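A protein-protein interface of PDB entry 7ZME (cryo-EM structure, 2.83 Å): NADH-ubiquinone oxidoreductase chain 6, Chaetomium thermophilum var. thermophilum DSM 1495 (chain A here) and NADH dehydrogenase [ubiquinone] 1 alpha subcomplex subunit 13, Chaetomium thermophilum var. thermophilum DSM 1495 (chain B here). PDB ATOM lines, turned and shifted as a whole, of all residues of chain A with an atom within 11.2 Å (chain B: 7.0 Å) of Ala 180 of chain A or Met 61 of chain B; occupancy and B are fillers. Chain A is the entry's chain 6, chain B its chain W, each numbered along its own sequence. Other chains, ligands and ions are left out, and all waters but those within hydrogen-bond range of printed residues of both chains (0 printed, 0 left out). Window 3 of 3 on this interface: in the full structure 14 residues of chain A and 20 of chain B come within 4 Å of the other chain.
O of Leu 179 of chain A sits at hydrogen-bond distance from NH2 of Arg 64 of chain B, at 2.8 Å.
OD1 of Asn 182 of chain A lies close to O of Ala 180 of chain A (2.9 Å).
Ile 68 of chain B touches Trp 175 of chain A.
Leu 179 of chain A touches Met 61 of chain B (CD1 to O, 3.9 Å).
Leu 179 of chain A touches Ile 65 of chain B.
Leu 179 of chain A touches Ile 68 of chain B (CD1 to CD1, 3.7 Å).
Ala 180 of chain A touches Met 61 of chain B (CB to SD, 3.9 Å).
Of chain B, only Met 61 (3.9 Å) comes within 4 Å of Ala 180 of chain A.
Met 61 of chain B touches two residues of chain A.
Ala 57 of chain B touches none of the printed residues of chain A.
No residue of chain A comes within 4 Å of Ala 63 of chain B.
Of the printed residues of chain B, Trp 175 of chain A touches Ile 68.
Of the printed residues of chain B, Leu 179 of chain A touches Met 61, Arg 64, Ile 65 and Ile 68.
Of the printed residues of chain A, Ile 68 of chain B touches Trp 175 and Leu 179.
His 184 of chain A touches none of the printed residues of chain B.
The nearest residue of chain A that does not touch Met 61 of chain B is Glu 181 of chain A (7.0 Å).
Of the 14 printed residues of chain A, 3 touch a printed residue of chain B.
Printed residues of chain A that touch a printed residue of chain B: Trp 175, Leu 179 and Ala 180.
Along chain A the printed residues that touch a printed residue of chain B span positions 175 to 180.
Hydrophobic or aromatic side chains of chain B within 4 Å of the printed part of chain A: Met 61, Ile 65 and Ile 68.
Among the printed residues, no Asp or Glu carboxylate lies within 4 Å of a Lys or Arg side-chain nitrogen of the other chain.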
ATOM      1  N   ILE A 174     -24.586  -7.498  14.088  1.00  0.00           N
ATOM      2  CA  ILE A 174     -24.273  -8.008  15.465  1.00  0.00           C
ATOM      3  C   ILE A 174     -23.122  -9.003  15.365  1.00  0.00           C
ATOM      4  O   ILE A 174     -22.945  -9.596  14.303  1.00  0.00           O
ATOM      5  CB  ILE A 174     -25.448  -8.627  16.255  1.00  0.00           C
ATOM      6  CG1 ILE A 174     -26.206  -9.694  15.464  1.00  0.00           C
ATOM      7  CG2 ILE A 174     -26.366  -7.557  16.828  1.00  0.00           C
ATOM      8  CD1 ILE A 174     -27.132 -10.523  16.320  1.00  0.00           C
ATOM      9  N   TRP A 175     -22.362  -9.140  16.442  1.00  0.00           N
ATOM     10  CA  TRP A 175     -21.185 -10.037  16.439  1.00  0.00           C
ATOM     11  C   TRP A 175     -21.454 -11.325  17.221  1.00  0.00           C
ATOM     12  O   TRP A 175     -21.004 -12.380  16.764  1.00  0.00           O
ATOM     13  CB  TRP A 175     -19.985  -9.240  16.956  1.00  0.00           C
ATOM     14  CG  TRP A 175     -19.653  -8.107  16.037  1.00  0.00           C
ATOM     15  CD1 TRP A 175     -19.961  -6.792  16.208  1.00  0.00           C
ATOM     16  CD2 TRP A 175     -18.993  -8.200  14.763  1.00  0.00           C
ATOM     17  NE1 TRP A 175     -19.513  -6.056  15.148  1.00  0.00           N
ATOM     18  CE2 TRP A 175     -18.918  -6.892  14.242  1.00  0.00           C
ATOM     19  CE3 TRP A 175     -18.447  -9.252  14.020  1.00  0.00           C
ATOM     20  CZ2 TRP A 175     -18.318  -6.614  13.016  1.00  0.00           C
ATOM     21  CZ3 TRP A 175     -17.857  -8.978  12.808  1.00  0.00           C
ATOM     22  CH2 TRP A 175     -17.792  -7.674  12.318  1.00  0.00           C
ATOM     23  N   ASP A 176     -22.164 -11.235  18.343  1.00  0.00           N
ATOM     24  CA  ASP A 176     -22.511 -12.422  19.172  1.00  0.00           C
ATOM     25  C   ASP A 176     -23.454 -13.370  18.417  1.00  0.00           C
ATOM     26  O   ASP A 176     -23.277 -14.592  18.530  1.00  0.00           O
ATOM     27  CB  ASP A 176     -22.967 -12.013  20.574  1.00  0.00           C
ATOM     28  CG  ASP A 176     -23.844 -10.773  20.613  1.00  0.00           C
ATOM     29  OD1 ASP A 176     -24.034 -10.230  21.719  1.00  0.00           O
ATOM     30  OD2 ASP A 176     -24.346 -10.367  19.549  1.00  0.00           O
ATOM     31  N   GLY A 177     -24.415 -12.829  17.677  1.00  0.00           N
ATOM     32  CA  GLY A 177     -25.365 -13.653  16.910  1.00  0.00           C
ATOM     33  C   GLY A 177     -24.830 -14.036  15.553  1.00  0.00           C
ATOM     34  O   GLY A 177     -25.522 -14.771  14.848  1.00  0.00           O
ATOM     35  N   ALA A 178     -23.652 -13.538  15.187  1.00  0.00           N
ATOM     36  CA  ALA A 178     -23.018 -13.920  13.906  1.00  0.00           C
ATOM     37  C   ALA A 178     -21.827 -14.853  14.119  1.00  0.00           C
ATOM     38  O   ALA A 178     -21.035 -14.973  13.175  1.00  0.00           O
ATOM     39  CB  ALA A 178     -22.597 -12.692  13.146  1.00  0.00           C
ATOM     40  N   LEU A 179     -21.670 -15.464  15.296  1.00  0.00           N
ATOM     41  CA  LEU A 179     -20.435 -16.265  15.498  1.00  0.00           C
ATOM     42  C   LEU A 179     -20.371 -17.426  14.501  1.00  0.00           C
ATOM     43  O   LEU A 179     -19.352 -17.544  13.816  1.00  0.00           O
ATOM     44  CB  LEU A 179     -20.420 -16.795  16.936  1.00  0.00           C
ATOM     45  CG  LEU A 179     -19.341 -17.831  17.245  1.00  0.00           C
ATOM     46  CD1 LEU A 179     -17.976 -17.181  17.381  1.00  0.00           C
ATOM     47  CD2 LEU A 179     -19.678 -18.604  18.504  1.00  0.00           C
ATOM     48  N   ALA A 180     -21.430 -18.223  14.396  1.00  0.00           N
ATOM     49  CA  ALA A 180     -21.482 -19.318  13.402  1.00  0.00           C
ATOM     50  C   ALA A 180     -22.842 -19.303  12.705  1.00  0.00           C
ATOM     51  O   ALA A 180     -23.622 -20.212  12.978  1.00  0.00           O
ATOM     52  CB  ALA A 180     -21.253 -20.620  14.104  1.00  0.00           C
ATOM     53  N   GLU A 181     -22.982 -18.279  11.721  1.00  0.00           N
ATOM     54  CA  GLU A 181     -24.293 -18.202  11.022  1.00  0.00           C
ATOM     55  C   GLU A 181     -24.601 -19.515  10.314  1.00  0.00           C
ATOM     56  O   GLU A 181     -23.693 -20.063   9.673  1.00  0.00           O
ATOM     57  CB  GLU A 181     -24.406 -17.009  10.079  1.00  0.00           C
ATOM     58  CG  GLU A 181     -25.655 -16.982   9.227  1.00  0.00           C
ATOM     59  CD  GLU A 181     -25.353 -16.602   7.790  1.00  0.00           C
ATOM     60  OE1 GLU A 181     -24.165 -16.404   7.479  1.00  0.00           O
ATOM     61  OE2 GLU A 181     -26.302 -16.512   6.988  1.00  0.00           O
ATOM     62  N   ASN A 182     -25.963 -20.004  10.534  1.00  0.00           N
ATOM     63  CA  ASN A 182     -26.299 -21.248   9.813  1.00  0.00           C
ATOM     64  C   ASN A 182     -27.074 -20.871   8.563  1.00  0.00           C
ATOM     65  O   ASN A 182     -27.611 -19.758   8.521  1.00  0.00           O
ATOM     66  CB  ASN A 182     -27.157 -22.188  10.664  1.00  0.00           C
ATOM     67  CG  ASN A 182     -26.474 -22.719  11.903  1.00  0.00           C
ATOM     68  OD1 ASN A 182     -25.324 -22.398  12.172  1.00  0.00           O
ATOM     69  ND2 ASN A 182     -27.180 -23.540  12.659  1.00  0.00           N
ATOM     70  N   ASN A 183     -27.126 -21.768   7.586  1.00  0.00           N
ATOM     71  CA  ASN A 183     -27.993 -21.531   6.406  1.00  0.00           C
ATOM     72  C   ASN A 183     -29.395 -21.906   6.875  1.00  0.00           C
ATOM     73  O   ASN A 183     -29.493 -22.612   7.879  1.00  0.00           O
ATOM     74  CB  ASN A 183     -27.512 -22.296   5.174  1.00  0.00           C
ATOM     75  CG  ASN A 183     -26.102 -21.931   4.765  1.00  0.00           C
ATOM     76  OD1 ASN A 183     -25.303 -22.801   4.432  1.00  0.00           O
ATOM     77  ND2 ASN A 183     -25.786 -20.647   4.799  1.00  0.00           N
ATOM     78  N   HIS A 184     -30.434 -21.464   6.183  1.00  0.00           N
ATOM     79  CA  HIS A 184     -31.816 -21.708   6.657  1.00  0.00           C
ATOM     80  C   HIS A 184     -32.094 -23.211   6.750  1.00  0.00           C
ATOM     81  O   HIS A 184     -32.776 -23.613   7.692  1.00  0.00           O
ATOM     82  CB  HIS A 184     -32.807 -20.999   5.735  1.00  0.00           C
ATOM     83  CG  HIS A 184     -32.832 -19.515   5.864  1.00  0.00           C
ATOM     84  ND1 HIS A 184     -33.748 -18.737   5.189  1.00  0.00           N
ATOM     85  CD2 HIS A 184     -32.068 -18.665   6.577  1.00  0.00           C
ATOM     86  CE1 HIS A 184     -33.547 -17.473   5.480  1.00  0.00           C
ATOM     87  NE2 HIS A 184     -32.521 -17.402   6.329  1.00  0.00           N
ATOM     88  N   SER A 186     -30.002 -25.575   7.411  1.00  0.00           N
ATOM     89  CA  SER A 186     -29.312 -26.053   8.633  1.00  0.00           C
ATOM     90  C   SER A 186     -30.117 -25.673   9.880  1.00  0.00           C
ATOM     91  O   SER A 186     -30.202 -26.493  10.792  1.00  0.00           O
ATOM     92  CB  SER A 186     -27.914 -25.539   8.678  1.00  0.00           C
ATOM     93  OG  SER A 186     -27.121 -26.333   9.543  1.00  0.00           O
ATOM     94  N   SER A 187     -30.693 -24.478   9.900  1.00  0.00           N
ATOM     95  CA  SER A 187     -31.512 -24.017  11.047  1.00  0.00           C
ATOM     96  C   SER A 187     -32.745 -24.904  11.204  1.00  0.00           C
ATOM     97  O   SER A 187     -33.128 -25.174  12.354  1.00  0.00           O
ATOM     98  CB  SER A 187     -31.880 -22.578  10.888  1.00  0.00           C
ATOM     99  OG  SER A 187     -30.741 -21.806  10.555  1.00  0.00           O
ATOM    100  N   ASN A 190     -31.595 -28.225  12.551  1.00  0.00           N
ATOM    101  CA  ASN A 190     -31.273 -28.172  13.972  1.00  0.00           C
ATOM    102  C   ASN A 190     -32.444 -28.591  14.851  1.00  0.00           C
ATOM    103  O   ASN A 190     -32.227 -29.043  15.979  1.00  0.00           O
ATOM    104  CB  ASN A 190     -30.827 -26.762  14.356  1.00  0.00           C
ATOM    105  CG  ASN A 190     -29.425 -26.433  13.878  1.00  0.00           C
ATOM    106  OD1 ASN A 190     -29.002 -25.280  13.918  1.00  0.00           O
ATOM    107  ND2 ASN A 190     -28.700 -27.443  13.422  1.00  0.00           N
ATOM    108  N   LEU B  56     -10.022 -27.896  13.279  1.00  0.00           N
ATOM    109  CA  LEU B  56      -9.795 -26.588  12.612  1.00  0.00           C
ATOM    110  C   LEU B  56     -10.999 -25.691  12.881  1.00  0.00           C
ATOM    111  O   LEU B  56     -10.802 -24.475  13.019  1.00  0.00           O
ATOM    112  CB  LEU B  56      -9.648 -26.838  11.109  1.00  0.00           C
ATOM    113  CG  LEU B  56      -8.345 -27.489  10.654  1.00  0.00           C
ATOM    114  CD1 LEU B  56      -8.344 -27.662   9.147  1.00  0.00           C
ATOM    115  CD2 LEU B  56      -7.154 -26.659  11.090  1.00  0.00           C
ATOM    116  N   ALA B  57     -12.198 -26.273  12.895  1.00  0.00           N
ATOM    117  CA  ALA B  57     -13.439 -25.525  13.199  1.00  0.00           C
ATOM    118  C   ALA B  57     -13.398 -24.987  14.630  1.00  0.00           C
ATOM    119  O   ALA B  57     -13.895 -23.877  14.842  1.00  0.00           O
ATOM    120  CB  ALA B  57     -14.630 -26.406  12.955  1.00  0.00           C
ATOM    121  N   ARG B  58     -12.844 -25.755  15.571  1.00  0.00           N
ATOM    122  CA  ARG B  58     -12.716 -25.309  16.984  1.00  0.00           C
ATOM    123  C   ARG B  58     -11.795 -24.092  17.070  1.00  0.00           C
ATOM    124  O   ARG B  58     -12.111 -23.177  17.836  1.00  0.00           O
ATOM    125  CB  ARG B  58     -12.180 -26.456  17.840  1.00  0.00           C
ATOM    126  CG  ARG B  58     -12.116 -26.154  19.329  1.00  0.00           C
ATOM    127  CD  ARG B  58     -11.398 -27.240  20.104  1.00  0.00           C
ATOM    128  NE  ARG B  58     -11.832 -28.568  19.707  1.00  0.00           N
ATOM    129  CZ  ARG B  58     -12.877 -29.210  20.214  1.00  0.00           C
ATOM    130  NH1 ARG B  58     -13.180 -30.417  19.774  1.00  0.00           N
ATOM    131  NH2 ARG B  58     -13.614 -28.647  21.154  1.00  0.00           N
ATOM    132  N   GLU B  59     -10.719 -24.071  16.287  1.00  0.00           N
ATOM    133  CA  GLU B  59      -9.739 -22.957  16.306  1.00  0.00           C
ATOM    134  C   GLU B  59     -10.377 -21.701  15.713  1.00  0.00           C
ATOM    135  O   GLU B  59     -10.178 -20.626  16.292  1.00  0.00           O
ATOM    136  CB  GLU B  59      -8.450 -23.427  15.644  1.00  0.00           C
ATOM    137  CG  GLU B  59      -7.377 -22.365  15.530  1.00  0.00           C
ATOM    138  CD  GLU B  59      -6.208 -22.836  14.688  1.00  0.00           C
ATOM    139  OE1 GLU B  59      -6.271 -23.970  14.191  1.00  0.00           O
ATOM    140  OE2 GLU B  59      -5.249 -22.070  14.520  1.00  0.00           O
ATOM    141  N   LYS B  60     -11.118 -21.841  14.612  1.00  0.00           N
ATOM    142  CA  LYS B  60     -11.806 -20.695  13.948  1.00  0.00           C
ATOM    143  C   LYS B  60     -12.843 -20.092  14.894  1.00  0.00           C
ATOM    144  O   LYS B  60     -13.056 -18.882  14.823  1.00  0.00           O
ATOM    145  CB  LYS B  60     -12.509 -21.156  12.672  1.00  0.00           C
ATOM    146  CG  LYS B  60     -13.156 -20.053  11.850  1.00  0.00           C
ATOM    147  CD  LYS B  60     -13.720 -20.536  10.541  1.00  0.00           C
ATOM    148  CE  LYS B  60     -14.138 -19.399   9.638  1.00  0.00           C
ATOM    149  NZ  LYS B  60     -14.386 -19.870   8.258  1.00  0.00           N
ATOM    150  N   MET B  61     -13.439 -20.908  15.762  1.00  0.00           N
ATOM    151  CA  MET B  61     -14.528 -20.416  16.632  1.00  0.00           C
ATOM    152  C   MET B  61     -13.941 -19.730  17.865  1.00  0.00           C
ATOM    153  O   MET B  61     -14.491 -18.698  18.238  1.00  0.00           O
ATOM    154  CB  MET B  61     -15.478 -21.545  17.041  1.00  0.00           C
ATOM    155  CG  MET B  61     -16.362 -22.056  15.914  1.00  0.00           C
ATOM    156  SD  MET B  61     -17.492 -20.822  15.217  1.00  0.00           S
ATOM    157  CE  MET B  61     -16.655 -20.398  13.691  1.00  0.00           C
ATOM    158  N   TRP B  62     -12.847 -20.249  18.434  1.00  0.00           N
ATOM    159  CA  TRP B  62     -12.196 -19.585  19.593  1.00  0.00           C
ATOM    160  C   TRP B  62     -11.562 -18.261  19.168  1.00  0.00           C
ATOM    161  O   TRP B  62     -11.610 -17.327  19.961  1.00  0.00           O
ATOM    162  CB  TRP B  62     -11.262 -20.534  20.347  1.00  0.00           C
ATOM    163  CG  TRP B  62     -12.009 -21.412  21.301  1.00  0.00           C
ATOM    164  CD1 TRP B  62     -12.333 -22.727  21.138  1.00  0.00           C
ATOM    165  CD2 TRP B  62     -12.573 -21.013  22.560  1.00  0.00           C
ATOM    166  NE1 TRP B  62     -13.039 -23.179  22.218  1.00  0.00           N
ATOM    167  CE2 TRP B  62     -13.209 -22.148  23.104  1.00  0.00           C
ATOM    168  CE3 TRP B  62     -12.592 -19.815  23.281  1.00  0.00           C
ATOM    169  CZ2 TRP B  62     -13.853 -22.115  24.337  1.00  0.00           C
ATOM    170  CZ3 TRP B  62     -13.230 -19.786  24.500  1.00  0.00           C
ATOM    171  CH2 TRP B  62     -13.847 -20.922  25.020  1.00  0.00           C
ATOM    172  N   ALA B  63     -11.013 -18.196  17.957  1.00  0.00           N
ATOM    173  CA  ALA B  63     -10.446 -16.938  17.424  1.00  0.00           C
ATOM    174  C   ALA B  63     -11.571 -15.914  17.279  1.00  0.00           C
ATOM    175  O   ALA B  63     -11.360 -14.752  17.658  1.00  0.00           O
ATOM    176  CB  ALA B  63      -9.793 -17.186  16.094  1.00  0.00           C
ATOM    177  N   ARG B  64     -12.712 -16.335  16.740  1.00  0.00           N
ATOM    178  CA  ARG B  64     -13.896 -15.447  16.625  1.00  0.00           C
ATOM    179  C   ARG B  64     -14.358 -15.003  18.015  1.00  0.00           C
ATOM    180  O   ARG B  64     -14.653 -13.821  18.159  1.00  0.00           O
ATOM    181  CB  ARG B  64     -14.984 -16.089  15.761  1.00  0.00           C
ATOM    182  CG  ARG B  64     -14.689 -16.085  14.270  1.00  0.00           C
ATOM    183  CD  ARG B  64     -15.895 -16.569  13.503  1.00  0.00           C
ATOM    184  NE  ARG B  64     -15.661 -16.459  12.075  1.00  0.00           N
ATOM    185  CZ  ARG B  64     -16.571 -16.705  11.150  1.00  0.00           C
ATOM    186  NH1 ARG B  64     -16.262 -16.574   9.872  1.00  0.00           N
ATOM    187  NH2 ARG B  64     -17.789 -17.068  11.503  1.00  0.00           N
ATOM    188  N   ILE B  65     -14.461 -15.919  18.974  1.00  0.00           N
ATOM    189  CA  ILE B  65     -14.968 -15.619  20.346  1.00  0.00           C
ATOM    190  C   ILE B  65     -14.141 -14.528  21.051  1.00  0.00           C
ATOM    191  O   ILE B  65     -14.759 -13.674  21.696  1.00  0.00           O
ATOM    192  CB  ILE B  65     -15.008 -16.924  21.168  1.00  0.00           C
ATOM    193  CG1 ILE B  65     -16.267 -17.741  20.875  1.00  0.00           C
ATOM    194  CG2 ILE B  65     -14.837 -16.665  22.657  1.00  0.00           C
ATOM    195  CD1 ILE B  65     -16.104 -19.216  21.138  1.00  0.00           C
ATOM    196  N   HIS B  66     -12.811 -14.526  20.924  1.00  0.00           N
ATOM    197  CA  HIS B  66     -11.986 -13.456  21.552  1.00  0.00           C
ATOM    198  C   HIS B  66     -12.327 -12.087  20.953  1.00  0.00           C
ATOM    199  O   HIS B  66     -12.256 -11.090  21.687  1.00  0.00           O
ATOM    200  CB  HIS B  66     -10.495 -13.799  21.504  1.00  0.00           C
ATOM    201  CG  HIS B  66     -10.142 -15.118  22.102  1.00  0.00           C
ATOM    202  ND1 HIS B  66     -10.617 -15.526  23.332  1.00  0.00           N
ATOM    203  CD2 HIS B  66      -9.342 -16.112  21.660  1.00  0.00           C
ATOM    204  CE1 HIS B  66     -10.139 -16.721  23.611  1.00  0.00           C
ATOM    205  NE2 HIS B  66      -9.354 -17.102  22.601  1.00  0.00           N
ATOM    206  N   ILE B  68     -15.279 -11.179  19.611  1.00  0.00           N
ATOM    207  CA  ILE B  68     -16.712 -10.805  19.781  1.00  0.00           C
ATOM    208  C   ILE B  68     -16.866  -9.682  20.804  1.00  0.00           C
ATOM    209  O   ILE B  68     -17.609  -8.747  20.488  1.00  0.00           O
ATOM    210  CB  ILE B  68     -17.570 -12.032  20.161  1.00  0.00           C
ATOM    211  CG1 ILE B  68     -17.856 -12.940  18.965  1.00  0.00           C
ATOM    212  CG2 ILE B  68     -18.858 -11.615  20.856  1.00  0.00           C
ATOM    213  CD1 ILE B  68     -18.742 -14.114  19.294  1.00  0.00           C
